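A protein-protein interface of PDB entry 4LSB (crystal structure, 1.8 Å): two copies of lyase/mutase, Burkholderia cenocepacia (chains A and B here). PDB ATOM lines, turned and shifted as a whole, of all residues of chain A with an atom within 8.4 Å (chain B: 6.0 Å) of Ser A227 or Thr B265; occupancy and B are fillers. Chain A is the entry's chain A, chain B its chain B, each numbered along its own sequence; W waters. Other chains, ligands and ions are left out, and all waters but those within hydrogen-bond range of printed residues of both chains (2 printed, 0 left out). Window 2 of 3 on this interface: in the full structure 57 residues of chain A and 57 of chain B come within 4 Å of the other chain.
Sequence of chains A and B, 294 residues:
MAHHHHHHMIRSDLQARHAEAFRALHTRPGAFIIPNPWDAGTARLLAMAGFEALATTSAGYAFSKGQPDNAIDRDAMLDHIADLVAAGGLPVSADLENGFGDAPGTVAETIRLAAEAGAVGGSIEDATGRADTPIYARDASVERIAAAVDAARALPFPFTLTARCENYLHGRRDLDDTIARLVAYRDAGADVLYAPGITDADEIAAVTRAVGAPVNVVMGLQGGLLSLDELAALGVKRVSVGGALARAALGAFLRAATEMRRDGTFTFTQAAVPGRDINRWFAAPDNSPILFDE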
ATOM      1  N   ALA A  31       4.131   5.633  26.686  1.00  0.00           N
ATOM      2  CA  ALA A  31       4.917   5.498  27.911  1.00  0.00           C
ATOM      3  C   ALA A  31       4.522   6.602  28.856  1.00  0.00           C
ATOM      4  O   ALA A  31       3.919   7.615  28.440  1.00  0.00           O
ATOM      5  CB  ALA A  31       6.388   5.580  27.606  1.00  0.00           C
ATOM      6  N   ILE A  33       5.911   8.773  32.616  1.00  0.00           N
ATOM      7  CA  ILE A  33       6.931   9.047  33.631  1.00  0.00           C
ATOM      8  C   ILE A  33       6.370   8.843  35.028  1.00  0.00           C
ATOM      9  O   ILE A  33       5.321   9.391  35.395  1.00  0.00           O
ATOM     10  CB  ILE A  33       7.464  10.496  33.510  1.00  0.00           C
ATOM     11  CG1 ILE A  33       8.147  10.694  32.144  1.00  0.00           C
ATOM     12  CG2 ILE A  33       8.370  10.818  34.652  1.00  0.00           C
ATOM     13  CD1 ILE A  33       8.477  12.138  31.856  1.00  0.00           C
ATOM     14  N   PHE A  51       1.609  14.981  37.372  1.00  0.00           N
ATOM     15  CA  PHE A  51       1.982  13.565  37.244  1.00  0.00           C
ATOM     16  C   PHE A  51       0.834  12.688  37.747  1.00  0.00           C
ATOM     17  O   PHE A  51       0.066  13.099  38.588  1.00  0.00           O
ATOM     18  CB  PHE A  51       3.305  13.260  37.969  1.00  0.00           C
ATOM     19  CG  PHE A  51       4.513  13.878  37.305  1.00  0.00           C
ATOM     20  CD1 PHE A  51       5.078  13.298  36.170  1.00  0.00           C
ATOM     21  CD2 PHE A  51       5.055  15.052  37.804  1.00  0.00           C
ATOM     22  CE1 PHE A  51       6.171  13.906  35.532  1.00  0.00           C
ATOM     23  CE2 PHE A  51       6.140  15.661  37.180  1.00  0.00           C
ATOM     24  CZ  PHE A  51       6.697  15.079  36.035  1.00  0.00           C
ATOM     25  N   ILE A 204      18.219  -1.408  25.309  1.00  0.00           N
ATOM     26  CA  ILE A 204      16.862  -1.234  25.797  1.00  0.00           C
ATOM     27  C   ILE A 204      15.876  -1.879  24.814  1.00  0.00           C
ATOM     28  O   ILE A 204      14.959  -2.591  25.230  1.00  0.00           O
ATOM     29  CB  ILE A 204      16.523   0.265  26.013  1.00  0.00           C
ATOM     30  CG1 ILE A 204      17.333   0.825  27.195  1.00  0.00           C
ATOM     31  CG2 ILE A 204      15.004   0.472  26.197  1.00  0.00           C
ATOM     32  CD1 ILE A 204      17.258   2.333  27.285  1.00  0.00           C
ATOM     33  N   VAL A 217      12.424   1.837  32.621  1.00  0.00           N
ATOM     34  CA  VAL A 217      13.813   2.308  32.469  1.00  0.00           C
ATOM     35  C   VAL A 217      13.999   3.512  33.368  1.00  0.00           C
ATOM     36  O   VAL A 217      13.160   4.423  33.403  1.00  0.00           O
ATOM     37  CB  VAL A 217      14.110   2.670  30.995  1.00  0.00           C
ATOM     38  CG1 VAL A 217      15.380   3.416  30.849  1.00  0.00           C
ATOM     39  CG2 VAL A 217      14.100   1.415  30.130  1.00  0.00           C
ATOM     40  N   MET A 219      16.224   6.878  34.282  1.00  0.00           N
ATOM     41  CA  MET A 219      17.036   7.893  33.661  1.00  0.00           C
ATOM     42  C   MET A 219      17.672   8.738  34.729  1.00  0.00           C
ATOM     43  O   MET A 219      16.988   9.166  35.677  1.00  0.00           O
ATOM     44  CB  MET A 219      16.153   8.776  32.758  1.00  0.00           C
ATOM     45  CG  MET A 219      15.896   8.187  31.359  1.00  0.00           C
ATOM     46  SD  MET A 219      17.478   8.062  30.454  1.00  0.00           S
ATOM     47  CE  MET A 219      17.636   6.341  29.994  1.00  0.00           C
ATOM     48  N   GLY A 224      23.965   7.352  29.626  1.00  0.00           N
ATOM     49  CA  GLY A 224      23.374   8.342  28.737  1.00  0.00           C
ATOM     50  C   GLY A 224      21.921   8.631  29.038  1.00  0.00           C
ATOM     51  O   GLY A 224      21.247   7.847  29.720  1.00  0.00           O
ATOM     52  N   LEU A 225      21.445   9.734  28.477  1.00  0.00           N
ATOM     53  CA  LEU A 225      20.064  10.100  28.564  1.00  0.00           C
ATOM     54  C   LEU A 225      19.279   9.955  27.265  1.00  0.00           C
ATOM     55  O   LEU A 225      19.794  10.137  26.148  1.00  0.00           O
ATOM     56  CB  LEU A 225      19.964  11.542  29.005  1.00  0.00           C
ATOM     57  CG  LEU A 225      20.570  11.953  30.324  1.00  0.00           C
ATOM     58  CD1 LEU A 225      20.441  13.475  30.481  1.00  0.00           C
ATOM     59  CD2 LEU A 225      19.890  11.205  31.446  1.00  0.00           C
ATOM     60  N   LEU A 226      18.021   9.592  27.432  1.00  0.00           N
ATOM     61  CA  LEU A 226      17.075   9.521  26.335  1.00  0.00           C
ATOM     62  C   LEU A 226      15.781  10.213  26.751  1.00  0.00           C
ATOM     63  O   LEU A 226      15.518  10.338  27.917  1.00  0.00           O
ATOM     64  CB  LEU A 226      16.818   8.062  26.003  1.00  0.00           C
ATOM     65  CG  LEU A 226      17.968   7.303  25.358  1.00  0.00           C
ATOM     66  CD1 LEU A 226      17.752   5.788  25.420  1.00  0.00           C
ATOM     67  CD2 LEU A 226      18.165   7.812  23.925  1.00  0.00           C
ATOM     68  N   SER A 227      15.010  10.737  25.797  1.00  0.00           N
ATOM     69  CA  SER A 227      13.750  11.386  26.136  1.00  0.00           C
ATOM     70  C   SER A 227      12.662  10.357  26.347  1.00  0.00           C
ATOM     71  O   SER A 227      12.819   9.177  25.966  1.00  0.00           O
ATOM     72  CB  SER A 227      13.340  12.345  25.021  1.00  0.00           C
ATOM     73  OG  SER A 227      12.995  11.598  23.873  1.00  0.00           O
ATOM     74  N   LEU A 228      11.540  10.768  26.956  1.00  0.00           N
ATOM     75  CA  LEU A 228      10.375   9.871  27.034  1.00  0.00           C
ATOM     76  C   LEU A 228       9.933   9.358  25.648  1.00  0.00           C
ATOM     77  O   LEU A 228       9.700   8.157  25.471  1.00  0.00           O
ATOM     78  CB  LEU A 228       9.209  10.563  27.690  1.00  0.00           C
ATOM     79  CG  LEU A 228       7.968   9.667  27.849  1.00  0.00           C
ATOM     80  CD1 LEU A 228       8.243   8.582  28.900  1.00  0.00           C
ATOM     81  CD2 LEU A 228       6.797  10.564  28.214  1.00  0.00           C
ATOM     82  N   ASP A 229       9.810  10.250  24.670  1.00  0.00           N
ATOM     83  CA  ASP A 229       9.523   9.807  23.284  1.00  0.00           C
ATOM     84  C   ASP A 229      10.498   8.763  22.736  1.00  0.00           C
ATOM     85  O   ASP A 229      10.066   7.760  22.135  1.00  0.00           O
ATOM     86  CB  ASP A 229       9.465  10.992  22.323  1.00  0.00           C
ATOM     87  CG  ASP A 229       8.249  11.828  22.529  1.00  0.00           C
ATOM     88  OD1 ASP A 229       7.279  11.348  23.144  1.00  0.00           O
ATOM     89  OD2 ASP A 229       8.262  12.993  22.096  1.00  0.00           O
ATOM     90  N   GLU A 230      11.794   9.009  22.892  1.00  0.00           N
ATOM     91  CA  GLU A 230      12.787   8.055  22.444  1.00  0.00           C
ATOM     92  C   GLU A 230      12.633   6.699  23.130  1.00  0.00           C
ATOM     93  O   GLU A 230      12.750   5.653  22.491  1.00  0.00           O
ATOM     94  CB  GLU A 230      14.190   8.587  22.666  1.00  0.00           C
ATOM     95  CG  GLU A 230      14.630   9.630  21.648  1.00  0.00           C
ATOM     96  CD  GLU A 230      15.936  10.301  22.029  1.00  0.00           C
ATOM     97  OE1 GLU A 230      16.162  10.662  23.213  1.00  0.00           O
ATOM     98  OE2 GLU A 230      16.760  10.478  21.112  1.00  0.00           O
ATOM     99  N   LEU A 231      12.369   6.720  24.429  1.00  0.00           N
ATOM    100  CA  LEU A 231      12.172   5.482  25.198  1.00  0.00           C
ATOM    101  C   LEU A 231      10.913   4.751  24.741  1.00  0.00           C
ATOM    102  O   LEU A 231      10.927   3.524  24.536  1.00  0.00           O
ATOM    103  CB  LEU A 231      12.147   5.793  26.710  1.00  0.00           C
ATOM    104  CG  LEU A 231      13.542   6.171  27.168  1.00  0.00           C
ATOM    105  CD1 LEU A 231      13.517   6.968  28.476  1.00  0.00           C
ATOM    106  CD2 LEU A 231      14.417   4.930  27.297  1.00  0.00           C
ATOM    107  N   ALA A 232       9.849   5.499  24.488  1.00  0.00           N
ATOM    108  CA  ALA A 232       8.600   4.847  24.053  1.00  0.00           C
ATOM    109  C   ALA A 232       8.777   4.194  22.676  1.00  0.00           C
ATOM    110  O   ALA A 232       8.311   3.091  22.434  1.00  0.00           O
ATOM    111  CB  ALA A 232       7.471   5.844  24.076  1.00  0.00           C
ATOM    112  N   ALA A 233       9.534   4.843  21.792  1.00  0.00           N
ATOM    113  CA  ALA A 233       9.889   4.270  20.471  1.00  0.00           C
ATOM    114  C   ALA A 233      10.724   3.028  20.573  1.00  0.00           C
ATOM    115  O   ALA A 233      10.716   2.211  19.644  1.00  0.00           O
ATOM    116  CB  ALA A 233      10.643   5.288  19.643  1.00  0.00           C
ATOM    117  N   LEU A 234      11.403   2.849  21.696  1.00  0.00           N
ATOM    118  CA  LEU A 234      12.182   1.613  21.990  1.00  0.00           C
ATOM    119  C   LEU A 234      11.351   0.552  22.725  1.00  0.00           C
ATOM    120  O   LEU A 234      11.856  -0.509  23.049  1.00  0.00           O
ATOM    121  CB  LEU A 234      13.416   1.922  22.818  1.00  0.00           C
ATOM    122  CG  LEU A 234      14.372   2.869  22.078  1.00  0.00           C
ATOM    123  CD1 LEU A 234      15.348   3.451  23.076  1.00  0.00           C
ATOM    124  CD2 LEU A 234      15.113   2.151  20.973  1.00  0.00           C
ATOM    125  N   VAL A 236       9.504   1.027  25.608  1.00  0.00           N
ATOM    126  CA  VAL A 236       9.496   1.190  27.055  1.00  0.00           C
ATOM    127  C   VAL A 236       8.125   1.690  27.475  1.00  0.00           C
ATOM    128  O   VAL A 236       7.547   2.478  26.776  1.00  0.00           O
ATOM    129  CB  VAL A 236      10.595   2.160  27.503  1.00  0.00           C
ATOM    130  CG1 VAL A 236      10.458   2.491  29.019  1.00  0.00           C
ATOM    131  CG2 VAL A 236      11.965   1.567  27.253  1.00  0.00           C
ATOM    132  N   VAL A 239       9.071   5.205  32.746  1.00  0.00           N
ATOM    133  CA  VAL A 239      10.365   5.840  32.917  1.00  0.00           C
ATOM    134  C   VAL A 239      10.345   6.521  34.279  1.00  0.00           C
ATOM    135  O   VAL A 239       9.449   7.370  34.551  1.00  0.00           O
ATOM    136  CB  VAL A 239      10.638   6.867  31.840  1.00  0.00           C
ATOM    137  CG1 VAL A 239      11.992   7.468  32.014  1.00  0.00           C
ATOM    138  CG2 VAL A 239      10.480   6.225  30.453  1.00  0.00           C
ATOM    139  N   VAL A 241      13.115   7.929  37.732  1.00  0.00           N
ATOM    140  CA  VAL A 241      14.375   8.652  37.903  1.00  0.00           C
ATOM    141  C   VAL A 241      15.167   8.283  39.171  1.00  0.00           C
ATOM    142  O   VAL A 241      16.231   8.836  39.421  1.00  0.00           O
ATOM    143  CB  VAL A 241      14.156  10.181  37.829  1.00  0.00           C
ATOM    144  CG1 VAL A 241      13.703  10.565  36.447  1.00  0.00           C
ATOM    145  CG2 VAL A 241      13.187  10.704  38.909  1.00  0.00           C
ATOM    146  N   ALA B 256      13.144  20.749  37.279  1.00  0.00           N
ATOM    147  CA  ALA B 256      13.214  19.359  36.783  1.00  0.00           C
ATOM    148  C   ALA B 256      11.816  18.813  36.469  1.00  0.00           C
ATOM    149  O   ALA B 256      11.607  18.188  35.403  1.00  0.00           O
ATOM    150  CB  ALA B 256      13.887  18.477  37.796  1.00  0.00           C
ATOM    151  N   GLU B 259      10.583  20.363  33.264  1.00  0.00           N
ATOM    152  CA  GLU B 259      11.238  19.819  32.086  1.00  0.00           C
ATOM    153  C   GLU B 259      10.571  18.490  31.772  1.00  0.00           C
ATOM    154  O   GLU B 259      10.197  18.203  30.605  1.00  0.00           O
ATOM    155  CB  GLU B 259      12.749  19.601  32.355  1.00  0.00           C
ATOM    156  CG  GLU B 259      13.447  19.017  31.143  1.00  0.00           C
ATOM    157  CD  GLU B 259      14.884  18.578  31.388  1.00  0.00           C
ATOM    158  OE1 GLU B 259      15.391  18.777  32.504  1.00  0.00           O
ATOM    159  OE2 GLU B 259      15.498  18.080  30.423  1.00  0.00           O
ATOM    160  N   MET B 260      10.357  17.649  32.799  1.00  0.00           N
ATOM    161  CA  MET B 260       9.771  16.352  32.531  1.00  0.00           C
ATOM    162  C   MET B 260       8.370  16.429  31.985  1.00  0.00           C
ATOM    163  O   MET B 260       8.022  15.666  31.041  1.00  0.00           O
ATOM    164  CB  MET B 260       9.806  15.437  33.754  1.00  0.00           C
ATOM    165  CG  MET B 260      11.231  14.985  34.084  1.00  0.00           C
ATOM    166  SD  MET B 260      11.204  13.840  35.480  1.00  0.00           S
ATOM    167  CE  MET B 260      10.869  14.924  36.842  1.00  0.00           C
ATOM    168  N   ASP B 263       8.699  18.619  28.316  1.00  0.00           N
ATOM    169  CA  ASP B 263       9.516  18.077  27.252  1.00  0.00           C
ATOM    170  C   ASP B 263       9.664  16.589  27.262  1.00  0.00           C
ATOM    171  O   ASP B 263      10.030  16.018  26.234  1.00  0.00           O
ATOM    172  CB  ASP B 263      10.908  18.738  27.254  1.00  0.00           C
ATOM    173  CG  ASP B 263      10.829  20.218  26.911  1.00  0.00           C
ATOM    174  OD1 ASP B 263       9.745  20.626  26.431  1.00  0.00           O
ATOM    175  OD2 ASP B 263      11.819  20.956  27.126  1.00  0.00           O
ATOM    176  N   GLY B 264       9.438  15.937  28.395  1.00  0.00           N
ATOM    177  CA  GLY B 264       9.755  14.502  28.521  1.00  0.00           C
ATOM    178  C   GLY B 264      11.246  14.200  28.558  1.00  0.00           C
ATOM    179  O   GLY B 264      11.666  13.114  28.187  1.00  0.00           O
ATOM    180  N   THR B 265      12.055  15.159  29.011  1.00  0.00           N
ATOM    181  CA  THR B 265      13.502  15.023  29.047  1.00  0.00           C
ATOM    182  C   THR B 265      14.028  15.129  30.500  1.00  0.00           C
ATOM    183  O   THR B 265      13.323  15.599  31.435  1.00  0.00           O
ATOM    184  CB  THR B 265      14.187  16.048  28.099  1.00  0.00           C
ATOM    185  OG1 THR B 265      13.752  17.398  28.416  1.00  0.00           O
ATOM    186  CG2 THR B 265      13.888  15.732  26.647  1.00  0.00           C
ATOM    187  N   PHE B 266      15.260  14.660  30.690  1.00  0.00           N
ATOM    188  CA  PHE B 266      15.857  14.486  31.984  1.00  0.00           C
ATOM    189  C   PHE B 266      17.222  15.149  32.113  1.00  0.00           C
ATOM    190  O   PHE B 266      18.106  14.701  32.887  1.00  0.00           O
ATOM    191  CB  PHE B 266      15.970  12.988  32.223  1.00  0.00           C
ATOM    192  CG  PHE B 266      14.654  12.258  32.077  1.00  0.00           C
ATOM    193  CD1 PHE B 266      13.733  12.262  33.108  1.00  0.00           C
ATOM    194  CD2 PHE B 266      14.321  11.617  30.901  1.00  0.00           C
ATOM    195  CE1 PHE B 266      12.526  11.615  32.998  1.00  0.00           C
ATOM    196  CE2 PHE B 266      13.107  10.979  30.773  1.00  0.00           C
ATOM    197  CZ  PHE B 266      12.203  10.974  31.831  1.00  0.00           C
ATOM    198  N   THR B 267      17.438  16.208  31.327  1.00  0.00           N
ATOM    199  CA  THR B 267      18.760  16.838  31.291  1.00  0.00           C
ATOM    200  C   THR B 267      19.069  17.533  32.623  1.00  0.00           C
ATOM    201  O   THR B 267      20.219  17.796  32.962  1.00  0.00           O
ATOM    202  CB  THR B 267      18.881  17.852  30.135  1.00  0.00           C
ATOM    203  OG1 THR B 267      17.968  18.954  30.321  1.00  0.00           O
ATOM    204  CG2 THR B 267      18.682  17.160  28.820  1.00  0.00           C
ATOM    205  N   PHE B 268      18.025  17.809  33.393  1.00  0.00           N
ATOM    206  CA  PHE B 268      18.240  18.297  34.725  1.00  0.00           C
ATOM    207  C   PHE B 268      19.222  17.424  35.573  1.00  0.00           C
ATOM    208  O   PHE B 268      19.834  17.894  36.501  1.00  0.00           O
ATOM    209  CB  PHE B 268      16.890  18.475  35.408  1.00  0.00           C
ATOM    210  CG  PHE B 268      16.271  17.195  35.883  1.00  0.00           C
ATOM    211  CD1 PHE B 268      16.717  16.574  37.052  1.00  0.00           C
ATOM    212  CD2 PHE B 268      15.236  16.622  35.180  1.00  0.00           C
ATOM    213  CE1 PHE B 268      16.114  15.442  37.514  1.00  0.00           C
ATOM    214  CE2 PHE B 268      14.648  15.422  35.619  1.00  0.00           C
ATOM    215  CZ  PHE B 268      15.077  14.860  36.804  1.00  0.00           C
HETATM  216  O   HOH W   1      16.407  13.158  28.428  1.00  0.00           O
HETATM  217  O   HOH W   2       9.799  13.336  25.056  1.00  0.00           O
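Of the 20 printed residues of chain A, 9 touch a printed residue of chain B. Hydrophobic or aromatic side chains of chain A within 4 Å of the printed part of chain B: Ile A33, Phe A51, Met A219, Leu A225, Leu A228, Val A239 and Val A241. Of the 9 printed residues of chain B, 5 touch a printed residue of chain A. Printed residues of chain B that touch a printed residue of chain A: Met B260, Gly B264, Thr B265, Phe B266 and Thr B267. Among the printed residues, 12 pairs touch across the chains. Among the printed residues, no Asp or Glu carboxylate lies within 4 Å of a Lys or Arg side-chain nitrogen of the other chain.
Among the printed residues, pairs that only touch across the chains: Ser A227 with Gly B264, Leu A226 with Phe B266, Val A239 with Phe B266, Leu A225 with Phe B266, Ile A33 with Met B260, Val A241 with Phe B266, Ser A227 with Thr B265, Met A219 with Phe B266, Leu A225 with Thr B267, Phe A51 with Met B260 and Ile A33 with Phe B266.
The backbone NH (N) of Leu A228 lies within hydrogen-bond range of the backbone carbonyl oxygen (O) of Gly B264 (2.7 Å).
Printed residues of chain B within 4 Å of Ile A33: Met B260 and Phe B266. Of the printed residues of chain B, Leu A226 touches Phe B266. Ser A227 touches just these residues of chain B: Gly B264 (3.4 Å) and Thr B265 (3.8 Å). Printed residues of chain B within 4 Å of Leu A228: Gly B264. Leu A234 touches none of the printed residues of chain B. Printed residues of chain B within 4 Å of Val A241: Phe B266 (3.7 Å). Ala B256 touches none of the printed residues of chain A. Of the printed residues of chain A, Met B260 touches Ile A33 and Phe A51. Of chain A, only Ser A227 (3.4 Å) and Leu A228 (2.7 Å) come within 4 Å of Gly B264. Printed residues of chain A within 4 Å of Thr B265: Ser A227.
Water W2 bridges O of Asp B263 and N of Asp A229. Water W1 lies within hydrogen-bond range of the backbone NH of Phe B266 (2.9 Å) and the backbone carbonyl oxygen of Leu A226 (3.0 Å).
The backbone NH of Ser A227 is in hydrogen-bond range of the side-chain carboxylate of Glu A230 (2.8 Å). O of Glu B259 is in hydrogen-bond range of N of Gly B264 (3.3 Å). The side-chain carboxylate of Glu B259 lies within hydrogen-bond range of the backbone NH of Phe B266 (3.4 Å). The side-chain sulfur (SD) of Met A219 sits at hydrogen-bond distance from the backbone NH (N) of Leu A226, 3.4 Å away. The side-chain hydroxyl of Thr B265 sits at hydrogen-bond distance from the side-chain carboxylate of Glu B259. The side-chain carboxylate (OE2) of Glu B259 lies within hydrogen-bond range of the side-chain hydroxyl (OG1) of Thr B267 (2.6 Å).
No position is printed for both chains. Of the 12 pairs that touch across the chains among the printed residues, none has its exchanged pair printed and touching as well.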
